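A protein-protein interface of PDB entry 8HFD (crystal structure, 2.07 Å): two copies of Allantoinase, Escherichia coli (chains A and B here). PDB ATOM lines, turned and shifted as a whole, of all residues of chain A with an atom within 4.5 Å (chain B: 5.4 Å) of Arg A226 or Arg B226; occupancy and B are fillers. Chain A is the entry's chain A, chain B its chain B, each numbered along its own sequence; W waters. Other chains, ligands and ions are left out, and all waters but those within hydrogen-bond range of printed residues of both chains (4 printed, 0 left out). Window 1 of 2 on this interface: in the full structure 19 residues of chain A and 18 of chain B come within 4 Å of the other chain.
CG2 of Thr A151 touches NH1 of Arg B226, at 3.0 Å. OE2 of Glu A222 touches CG of Arg B226 (3.7 Å). Glu A222 touches Tyr B229. NH2 of Arg B225 touches NH2 of Arg A225, at 3.5 Å. Arg A226 touches Glu B222. Arg A226 touches Arg B226. CG1 of Val B221 touches OH of Tyr A229, at 3.3 Å. Tyr A229 touches Glu B222.
Asp A166 touches Arg B226, and with the chains exchanged Arg A226 touches Asp B166. Glu A222 touches Tyr B229, and with the chains exchanged Tyr A229 touches Glu B222. Arg B225 touches its own counterpart, Arg A225. Arg A226 touches its own counterpart, Arg B226. Of the 13 pairs that touch across the chains among the printed residues, 10 have their exchanged pair printed and touching as well.
Of chain B, only Asp B166 (2.7 Å), Glu B222 (3.8 Å) and Arg B226 (3.5 Å) come within 4 Å of Arg A226. Printed residues of chain A within 4 Å of Tyr B229: Glu A222. Printed residues of chain B within 4 Å of Glu A222: Arg B226 (3.7 Å) and Tyr B229 (3.7 Å). Of the printed residues of chain B, Thr A151 touches Asp B166 (3.1 Å) and Arg B226 (3.0 Å). Of the printed residues of chain A, Asn B189 touches Asp A166 (2.9 Å). Of the printed residues of chain B, Arg A225 touches Arg B225 (3.5 Å). The nearest printed residue of chain B that does not touch Arg A226 is Asn B189 (6.1 Å). The nearest printed residue of chain A that does not touch Arg B226 is Asn A189 (6.0 Å).
Water W4 lies within hydrogen-bond range of O of Arg B225 (2.7 Å) and NH2 of Arg A225 (2.8 Å). Water W1 lies within hydrogen-bond range of the guanidinium group (NH2) of Arg B225 (2.7 Å) and the backbone carbonyl oxygen (O) of Arg A225 (2.8 Å). Water W3 lies within hydrogen-bond range of the backbone carbonyl oxygen (O) of Arg A225 (2.8 Å) and the guanidinium group (NE) of Arg B225 (3.0 Å). Water W2 lies within hydrogen-bond range of NE of Arg A225 and O of Arg B225.
The side-chain carboxylate (OE2) of Glu A222 is in salt-bridge range of the guanidinium group (NE) of Arg A226. The side-chain carboxylate (OD1) of Asp B166 is in salt-bridge range of the guanidinium group (NH1) of Arg B226, at 3.2 Å. The side-chain amide nitrogen (ND2) of Asn B189 sits at hydrogen-bond distance from the side-chain carboxylate (OE1) of Glu B222, at 2.9 Å. The side-chain amide nitrogen (ND2) of Asn A189 sits close to the guanidinium group (NH2) of Arg A226 (3.3 Å). OE2 of Glu B222 is in salt-bridge range of NE of Arg B226. The guanidinium group (NH1) of Arg A226 lies within salt-bridge range of the side-chain carboxylate (OD1) of Asp A166 (3.1 Å).
The side-chain carboxylate (OD2) of Asp B166 lies within salt-bridge range of the guanidinium group (NH2) of Arg A226, at 2.7 Å. NH2 of Arg B226 is in salt-bridge range of OD2 of Asp A166. The side-chain hydroxyl (OG1) of Thr A151 sits at hydrogen-bond distance from the side-chain carboxylate (OD2) of Asp B166 (3.1 Å). The side-chain amide nitrogen (ND2) of Asn A189 is in hydrogen-bond range of the side-chain carboxylate (OD2) of Asp B166 (3.0 Å). The side-chain carboxylate (OD2) of Asp A166 lies within hydrogen-bond range of the side-chain amide nitrogen (ND2) of Asn B189.
Of the 12 printed residues of chain A, 7 touch a printed residue of chain B. Hydrophobic or aromatic side chains of chain A that line the printed part of chain B: Tyr A229. Among the printed residues, 13 pairs touch across the chains. Among the printed residues, Asp or Glu carboxylates within 4 Å of a Lys or Arg side-chain nitrogen of the other chain: Asp A166 with Arg B226 (2.8 Å) and Arg A226 with Asp B166 (2.7 Å).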
ATOM      1  N   THR A 151     -11.141  -8.424  14.659  1.00  0.00           N
ATOM      2  CA  THR A 151     -10.324  -8.783  13.475  1.00  0.00           C
ATOM      3  C   THR A 151     -10.659  -7.728  12.423  1.00  0.00           C
ATOM      4  O   THR A 151      -9.721  -7.247  11.774  1.00  0.00           O
ATOM      5  CB  THR A 151     -10.795 -10.148  12.958  1.00  0.00           C
ATOM      6  OG1 THR A 151     -11.300 -10.931  14.042  1.00  0.00           O
ATOM      7  CG2 THR A 151      -9.709 -10.904  12.225  1.00  0.00           C
ATOM      8  N   ASP A 166      -6.534  -6.322  14.037  1.00  0.00           N
ATOM      9  CA  ASP A 166      -5.285  -7.016  14.448  1.00  0.00           C
ATOM     10  C   ASP A 166      -4.063  -6.139  14.153  1.00  0.00           C
ATOM     11  O   ASP A 166      -3.156  -6.093  14.980  1.00  0.00           O
ATOM     12  CB  ASP A 166      -5.166  -8.385  13.773  1.00  0.00           C
ATOM     13  CG  ASP A 166      -6.266  -9.374  14.135  1.00  0.00           C
ATOM     14  OD1 ASP A 166      -6.944  -9.161  15.156  1.00  0.00           O
ATOM     15  OD2 ASP A 166      -6.433 -10.350  13.390  1.00  0.00           O
ATOM     16  N   ASN A 189     -14.315 -12.711  21.186  1.00  0.00           N
ATOM     17  CA  ASN A 189     -14.450 -12.640  19.707  1.00  0.00           C
ATOM     18  C   ASN A 189     -15.821 -12.012  19.438  1.00  0.00           C
ATOM     19  O   ASN A 189     -16.813 -12.738  19.499  1.00  0.00           O
ATOM     20  CB  ASN A 189     -14.205 -13.990  19.032  1.00  0.00           C
ATOM     21  CG  ASN A 189     -14.117 -13.894  17.526  1.00  0.00           C
ATOM     22  OD1 ASN A 189     -15.088 -13.552  16.861  1.00  0.00           O
ATOM     23  ND2 ASN A 189     -12.954 -14.205  16.981  1.00  0.00           N
ATOM     24  N   GLU A 222     -10.416 -17.819  22.669  1.00  0.00           N
ATOM     25  CA  GLU A 222      -9.817 -17.460  21.383  1.00  0.00           C
ATOM     26  C   GLU A 222      -9.255 -16.051  21.422  1.00  0.00           C
ATOM     27  O   GLU A 222      -8.155 -15.788  20.913  1.00  0.00           O
ATOM     28  CB  GLU A 222     -10.851 -17.570  20.252  1.00  0.00           C
ATOM     29  CG  GLU A 222     -10.227 -17.425  18.855  1.00  0.00           C
ATOM     30  CD  GLU A 222      -9.928 -15.968  18.457  1.00  0.00           C
ATOM     31  OE1 GLU A 222     -10.727 -15.086  18.799  1.00  0.00           O
ATOM     32  OE2 GLU A 222      -8.888 -15.710  17.794  1.00  0.00           O
ATOM     33  N   ALA A 223     -10.009 -15.113  21.990  1.00  0.00           N
ATOM     34  CA  ALA A 223      -9.567 -13.721  21.969  1.00  0.00           C
ATOM     35  C   ALA A 223      -8.350 -13.518  22.867  1.00  0.00           C
ATOM     36  O   ALA A 223      -7.415 -12.792  22.506  1.00  0.00           O
ATOM     37  CB  ALA A 223     -10.726 -12.803  22.373  1.00  0.00           C
ATOM     38  N   ILE A 224      -8.335 -14.170  24.030  1.00  0.00           N
ATOM     39  CA  ILE A 224      -7.167 -14.104  24.908  1.00  0.00           C
ATOM     40  C   ILE A 224      -5.948 -14.699  24.217  1.00  0.00           C
ATOM     41  O   ILE A 224      -4.870 -14.108  24.220  1.00  0.00           O
ATOM     42  CB  ILE A 224      -7.464 -14.800  26.248  1.00  0.00           C
ATOM     43  CG1 ILE A 224      -8.470 -13.964  27.057  1.00  0.00           C
ATOM     44  CG2 ILE A 224      -6.184 -14.984  27.048  1.00  0.00           C
ATOM     45  CD1 ILE A 224      -9.143 -14.745  28.188  1.00  0.00           C
ATOM     46  N   ARG A 225      -6.106 -15.861  23.581  1.00  0.00           N
ATOM     47  CA  ARG A 225      -4.963 -16.470  22.908  1.00  0.00           C
ATOM     48  C   ARG A 225      -4.445 -15.579  21.786  1.00  0.00           C
ATOM     49  O   ARG A 225      -3.230 -15.474  21.587  1.00  0.00           O
ATOM     50  CB  ARG A 225      -5.331 -17.844  22.360  1.00  0.00           C
ATOM     51  CG  ARG A 225      -5.451 -18.914  23.430  1.00  0.00           C
ATOM     52  CD  ARG A 225      -6.006 -20.221  22.855  1.00  0.00           C
ATOM     53  NE  ARG A 225      -5.085 -20.907  21.945  1.00  0.00           N
ATOM     54  CZ  ARG A 225      -4.030 -21.614  22.328  1.00  0.00           C
ATOM     55  NH1 ARG A 225      -3.658 -21.673  23.603  1.00  0.00           N
ATOM     56  NH2 ARG A 225      -3.333 -22.290  21.413  1.00  0.00           N
ATOM     57  N   ARG A 226      -5.346 -14.932  21.042  1.00  0.00           N
ATOM     58  CA  ARG A 226      -4.903 -14.084  19.944  1.00  0.00           C
ATOM     59  C   ARG A 226      -4.124 -12.885  20.468  1.00  0.00           C
ATOM     60  O   ARG A 226      -3.039 -12.571  19.974  1.00  0.00           O
ATOM     61  CB  ARG A 226      -6.096 -13.635  19.107  1.00  0.00           C
ATOM     62  CG  ARG A 226      -5.735 -12.701  17.981  1.00  0.00           C
ATOM     63  CD  ARG A 226      -6.971 -11.930  17.490  1.00  0.00           C
ATOM     64  NE  ARG A 226      -8.032 -12.847  17.093  1.00  0.00           N
ATOM     65  CZ  ARG A 226      -9.025 -12.534  16.271  1.00  0.00           C
ATOM     66  NH1 ARG A 226      -9.124 -11.322  15.737  1.00  0.00           N
ATOM     67  NH2 ARG A 226      -9.936 -13.458  15.969  1.00  0.00           N
ATOM     68  N   VAL A 227      -4.652 -12.241  21.510  1.00  0.00           N
ATOM     69  CA  VAL A 227      -4.032 -11.051  22.083  1.00  0.00           C
ATOM     70  C   VAL A 227      -2.744 -11.406  22.824  1.00  0.00           C
ATOM     71  O   VAL A 227      -1.725 -10.719  22.683  1.00  0.00           O
ATOM     72  CB  VAL A 227      -5.065 -10.343  22.987  1.00  0.00           C
ATOM     73  CG1 VAL A 227      -4.396  -9.528  24.029  1.00  0.00           C
ATOM     74  CG2 VAL A 227      -5.973  -9.447  22.111  1.00  0.00           C
ATOM     75  N   LEU A 228      -2.754 -12.493  23.603  1.00  0.00           N
ATOM     76  CA  LEU A 228      -1.516 -12.953  24.236  1.00  0.00           C
ATOM     77  C   LEU A 228      -0.368 -13.013  23.229  1.00  0.00           C
ATOM     78  O   LEU A 228       0.734 -12.499  23.484  1.00  0.00           O
ATOM     79  CB  LEU A 228      -1.734 -14.327  24.861  1.00  0.00           C
ATOM     80  CG  LEU A 228      -2.299 -14.396  26.278  1.00  0.00           C
ATOM     81  CD1 LEU A 228      -2.649 -15.823  26.548  1.00  0.00           C
ATOM     82  CD2 LEU A 228      -1.252 -13.884  27.299  1.00  0.00           C
ATOM     83  N   TYR A 229      -0.622 -13.641  22.072  1.00  0.00           N
ATOM     84  CA  TYR A 229       0.436 -13.856  21.082  1.00  0.00           C
ATOM     85  C   TYR A 229       0.843 -12.558  20.388  1.00  0.00           C
ATOM     86  O   TYR A 229       2.033 -12.317  20.173  1.00  0.00           O
ATOM     87  CB  TYR A 229       0.007 -14.901  20.040  1.00  0.00           C
ATOM     88  CG  TYR A 229       1.115 -15.206  19.042  1.00  0.00           C
ATOM     89  CD1 TYR A 229       2.268 -15.892  19.448  1.00  0.00           C
ATOM     90  CD2 TYR A 229       1.044 -14.759  17.722  1.00  0.00           C
ATOM     91  CE1 TYR A 229       3.305 -16.153  18.559  1.00  0.00           C
ATOM     92  CE2 TYR A 229       2.093 -15.015  16.804  1.00  0.00           C
ATOM     93  CZ  TYR A 229       3.220 -15.718  17.243  1.00  0.00           C
ATOM     94  OH  TYR A 229       4.271 -15.978  16.377  1.00  0.00           O
ATOM     95  N   LEU A 230      -0.120 -11.713  20.014  1.00  0.00           N
ATOM     96  CA  LEU A 230       0.233 -10.470  19.330  1.00  0.00           C
ATOM     97  C   LEU A 230       0.984  -9.513  20.244  1.00  0.00           C
ATOM     98  O   LEU A 230       1.920  -8.817  19.809  1.00  0.00           O
ATOM     99  CB  LEU A 230      -1.035  -9.797  18.778  1.00  0.00           C
ATOM    100  CG  LEU A 230      -1.655 -10.485  17.556  1.00  0.00           C
ATOM    101  CD1 LEU A 230      -2.859  -9.696  16.977  1.00  0.00           C
ATOM    102  CD2 LEU A 230      -0.580 -10.694  16.482  1.00  0.00           C
ATOM    103  N   ALA B 150     -10.067 -14.411   7.107  1.00  0.00           N
ATOM    104  CA  ALA B 150      -9.901 -12.941   7.223  1.00  0.00           C
ATOM    105  C   ALA B 150      -8.435 -12.526   7.057  1.00  0.00           C
ATOM    106  O   ALA B 150      -7.761 -12.375   8.095  1.00  0.00           O
ATOM    107  CB  ALA B 150     -10.479 -12.474   8.540  1.00  0.00           C
ATOM    108  N   ASP B 166     -14.256 -14.921  10.963  1.00  0.00           N
ATOM    109  CA  ASP B 166     -14.138 -15.929  12.018  1.00  0.00           C
ATOM    110  C   ASP B 166     -15.450 -16.696  12.220  1.00  0.00           C
ATOM    111  O   ASP B 166     -15.437 -17.909  12.461  1.00  0.00           O
ATOM    112  CB  ASP B 166     -13.703 -15.276  13.332  1.00  0.00           C
ATOM    113  CG  ASP B 166     -12.256 -14.751  13.303  1.00  0.00           C
ATOM    114  OD1 ASP B 166     -11.474 -15.100  12.393  1.00  0.00           O
ATOM    115  OD2 ASP B 166     -11.901 -13.985  14.226  1.00  0.00           O
ATOM    116  N   ASN B 189      -2.340 -14.205   8.671  1.00  0.00           N
ATOM    117  CA  ASN B 189      -3.120 -13.035   9.051  1.00  0.00           C
ATOM    118  C   ASN B 189      -3.020 -12.028   7.907  1.00  0.00           C
ATOM    119  O   ASN B 189      -2.040 -11.289   7.787  1.00  0.00           O
ATOM    120  CB  ASN B 189      -2.640 -12.445  10.377  1.00  0.00           C
ATOM    121  CG  ASN B 189      -3.605 -11.398  10.901  1.00  0.00           C
ATOM    122  OD1 ASN B 189      -3.888 -10.406  10.215  1.00  0.00           O
ATOM    123  ND2 ASN B 189      -4.191 -11.659  12.065  1.00  0.00           N
ATOM    124  N   VAL B 221       2.025 -17.969  12.176  1.00  0.00           N
ATOM    125  CA  VAL B 221       1.787 -18.641  13.446  1.00  0.00           C
ATOM    126  C   VAL B 221       0.441 -18.215  14.028  1.00  0.00           C
ATOM    127  O   VAL B 221      -0.355 -19.048  14.466  1.00  0.00           O
ATOM    128  CB  VAL B 221       2.943 -18.370  14.426  1.00  0.00           C
ATOM    129  CG1 VAL B 221       2.533 -18.791  15.840  1.00  0.00           C
ATOM    130  CG2 VAL B 221       4.218 -19.143  13.973  1.00  0.00           C
ATOM    131  N   GLU B 222       0.161 -16.911  14.042  1.00  0.00           N
ATOM    132  CA  GLU B 222      -1.116 -16.458  14.593  1.00  0.00           C
ATOM    133  C   GLU B 222      -2.286 -17.111  13.871  1.00  0.00           C
ATOM    134  O   GLU B 222      -3.239 -17.587  14.504  1.00  0.00           O
ATOM    135  CB  GLU B 222      -1.251 -14.934  14.506  1.00  0.00           C
ATOM    136  CG  GLU B 222      -2.460 -14.397  15.289  1.00  0.00           C
ATOM    137  CD  GLU B 222      -3.801 -14.580  14.561  1.00  0.00           C
ATOM    138  OE1 GLU B 222      -3.879 -14.237  13.357  1.00  0.00           O
ATOM    139  OE2 GLU B 222      -4.774 -15.050  15.190  1.00  0.00           O
ATOM    140  N   ALA B 223      -2.251 -17.109  12.537  1.00  0.00           N
ATOM    141  CA  ALA B 223      -3.384 -17.639  11.794  1.00  0.00           C
ATOM    142  C   ALA B 223      -3.521 -19.128  12.046  1.00  0.00           C
ATOM    143  O   ALA B 223      -4.631 -19.639  12.256  1.00  0.00           O
ATOM    144  CB  ALA B 223      -3.231 -17.337  10.300  1.00  0.00           C
ATOM    145  N   ILE B 224      -2.398 -19.841  12.079  1.00  0.00           N
ATOM    146  CA  ILE B 224      -2.457 -21.264  12.389  1.00  0.00           C
ATOM    147  C   ILE B 224      -3.039 -21.480  13.782  1.00  0.00           C
ATOM    148  O   ILE B 224      -3.879 -22.367  13.985  1.00  0.00           O
ATOM    149  CB  ILE B 224      -1.073 -21.922  12.260  1.00  0.00           C
ATOM    150  CG1 ILE B 224      -0.655 -22.030  10.794  1.00  0.00           C
ATOM    151  CG2 ILE B 224      -1.088 -23.330  12.896  1.00  0.00           C
ATOM    152  CD1 ILE B 224       0.807 -22.465  10.652  1.00  0.00           C
ATOM    153  N   ARG B 225      -2.582 -20.699  14.774  1.00  0.00           N
ATOM    154  CA  ARG B 225      -3.093 -20.915  16.122  1.00  0.00           C
ATOM    155  C   ARG B 225      -4.584 -20.631  16.187  1.00  0.00           C
ATOM    156  O   ARG B 225      -5.331 -21.338  16.878  1.00  0.00           O
ATOM    157  CB  ARG B 225      -2.331 -20.065  17.129  1.00  0.00           C
ATOM    158  CG  ARG B 225      -0.990 -20.668  17.488  1.00  0.00           C
ATOM    159  CD  ARG B 225      -0.092 -19.643  18.134  1.00  0.00           C
ATOM    160  NE  ARG B 225      -0.566 -19.311  19.472  1.00  0.00           N
ATOM    161  CZ  ARG B 225      -0.508 -20.121  20.515  1.00  0.00           C
ATOM    162  NH1 ARG B 225       0.005 -21.337  20.418  1.00  0.00           N
ATOM    163  NH2 ARG B 225      -0.981 -19.700  21.691  1.00  0.00           N
ATOM    164  N   ARG B 226      -5.037 -19.615  15.463  1.00  0.00           N
ATOM    165  CA  ARG B 226      -6.455 -19.286  15.450  1.00  0.00           C
ATOM    166  C   ARG B 226      -7.271 -20.399  14.805  1.00  0.00           C
ATOM    167  O   ARG B 226      -8.293 -20.828  15.356  1.00  0.00           O
ATOM    168  CB  ARG B 226      -6.687 -17.957  14.716  1.00  0.00           C
ATOM    169  CG  ARG B 226      -8.141 -17.530  14.679  1.00  0.00           C
ATOM    170  CD  ARG B 226      -8.370 -16.341  13.742  1.00  0.00           C
ATOM    171  NE  ARG B 226      -7.429 -15.244  13.958  1.00  0.00           N
ATOM    172  CZ  ARG B 226      -7.590 -14.019  13.464  1.00  0.00           C
ATOM    173  NH1 ARG B 226      -8.634 -13.708  12.709  1.00  0.00           N
ATOM    174  NH2 ARG B 226      -6.682 -13.080  13.735  1.00  0.00           N
ATOM    175  N   VAL B 227      -6.850 -20.883  13.629  1.00  0.00           N
ATOM    176  CA  VAL B 227      -7.709 -21.858  12.969  1.00  0.00           C
ATOM    177  C   VAL B 227      -7.617 -23.218  13.676  1.00  0.00           C
ATOM    178  O   VAL B 227      -8.596 -23.976  13.697  1.00  0.00           O
ATOM    179  CB  VAL B 227      -7.418 -21.962  11.450  1.00  0.00           C
ATOM    180  CG1 VAL B 227      -7.536 -20.602  10.747  1.00  0.00           C
ATOM    181  CG2 VAL B 227      -6.075 -22.572  11.168  1.00  0.00           C
ATOM    182  N   LEU B 228      -6.467 -23.548  14.282  1.00  0.00           N
ATOM    183  CA  LEU B 228      -6.374 -24.781  15.075  1.00  0.00           C
ATOM    184  C   LEU B 228      -7.424 -24.802  16.188  1.00  0.00           C
ATOM    185  O   LEU B 228      -8.108 -25.809  16.406  1.00  0.00           O
ATOM    186  CB  LEU B 228      -4.976 -24.924  15.685  1.00  0.00           C
ATOM    187  CG  LEU B 228      -3.800 -25.510  14.897  1.00  0.00           C
ATOM    188  CD1 LEU B 228      -2.505 -25.206  15.635  1.00  0.00           C
ATOM    189  CD2 LEU B 228      -3.959 -27.023  14.681  1.00  0.00           C
ATOM    190  N   TYR B 229      -7.560 -23.684  16.908  1.00  0.00           N
ATOM    191  CA  TYR B 229      -8.506 -23.625  18.011  1.00  0.00           C
ATOM    192  C   TYR B 229      -9.950 -23.594  17.514  1.00  0.00           C
ATOM    193  O   TYR B 229     -10.808 -24.303  18.050  1.00  0.00           O
ATOM    194  CB  TYR B 229      -8.217 -22.416  18.903  1.00  0.00           C
ATOM    195  CG  TYR B 229      -9.101 -22.398  20.131  1.00  0.00           C
ATOM    196  CD1 TYR B 229      -9.036 -23.424  21.072  1.00  0.00           C
ATOM    197  CD2 TYR B 229     -10.010 -21.364  20.344  1.00  0.00           C
ATOM    198  CE1 TYR B 229      -9.851 -23.425  22.193  1.00  0.00           C
ATOM    199  CE2 TYR B 229     -10.829 -21.349  21.483  1.00  0.00           C
ATOM    200  CZ  TYR B 229     -10.739 -22.384  22.388  1.00  0.00           C
ATOM    201  OH  TYR B 229     -11.549 -22.389  23.477  1.00  0.00           O
ATOM    202  N   LEU B 230     -10.250 -22.770  16.501  1.00  0.00           N
ATOM    203  CA  LEU B 230     -11.620 -22.741  16.000  1.00  0.00           C
ATOM    204  C   LEU B 230     -12.027 -24.102  15.421  1.00  0.00           C
ATOM    205  O   LEU B 230     -13.141 -24.583  15.671  1.00  0.00           O
ATOM    206  CB  LEU B 230     -11.794 -21.620  14.975  1.00  0.00           C
ATOM    207  CG  LEU B 230     -11.833 -20.202  15.580  1.00  0.00           C
ATOM    208  CD1 LEU B 230     -11.972 -19.141  14.499  1.00  0.00           C
ATOM    209  CD2 LEU B 230     -12.948 -20.035  16.621  1.00  0.00           C
ATOM    210  N   ALA B 231     -11.134 -24.753  14.670  1.00  0.00           N
ATOM    211  CA  ALA B 231     -11.452 -26.092  14.157  1.00  0.00           C
ATOM    212  C   ALA B 231     -11.679 -27.095  15.289  1.00  0.00           C
ATOM    213  O   ALA B 231     -12.573 -27.942  15.203  1.00  0.00           O
ATOM    214  CB  ALA B 231     -10.341 -26.598  13.242  1.00  0.00           C
HETATM  215  O   HOH W   1      -1.462 -17.258  22.758  1.00  0.00           O
HETATM  216  O   HOH W   2      -5.871 -19.760  19.349  1.00  0.00           O
HETATM  217  O   HOH W   3      -2.613 -17.133  19.369  1.00  0.00           O
HETATM  218  O   HOH W   4      -4.271 -22.835  18.814  1.00  0.00           O
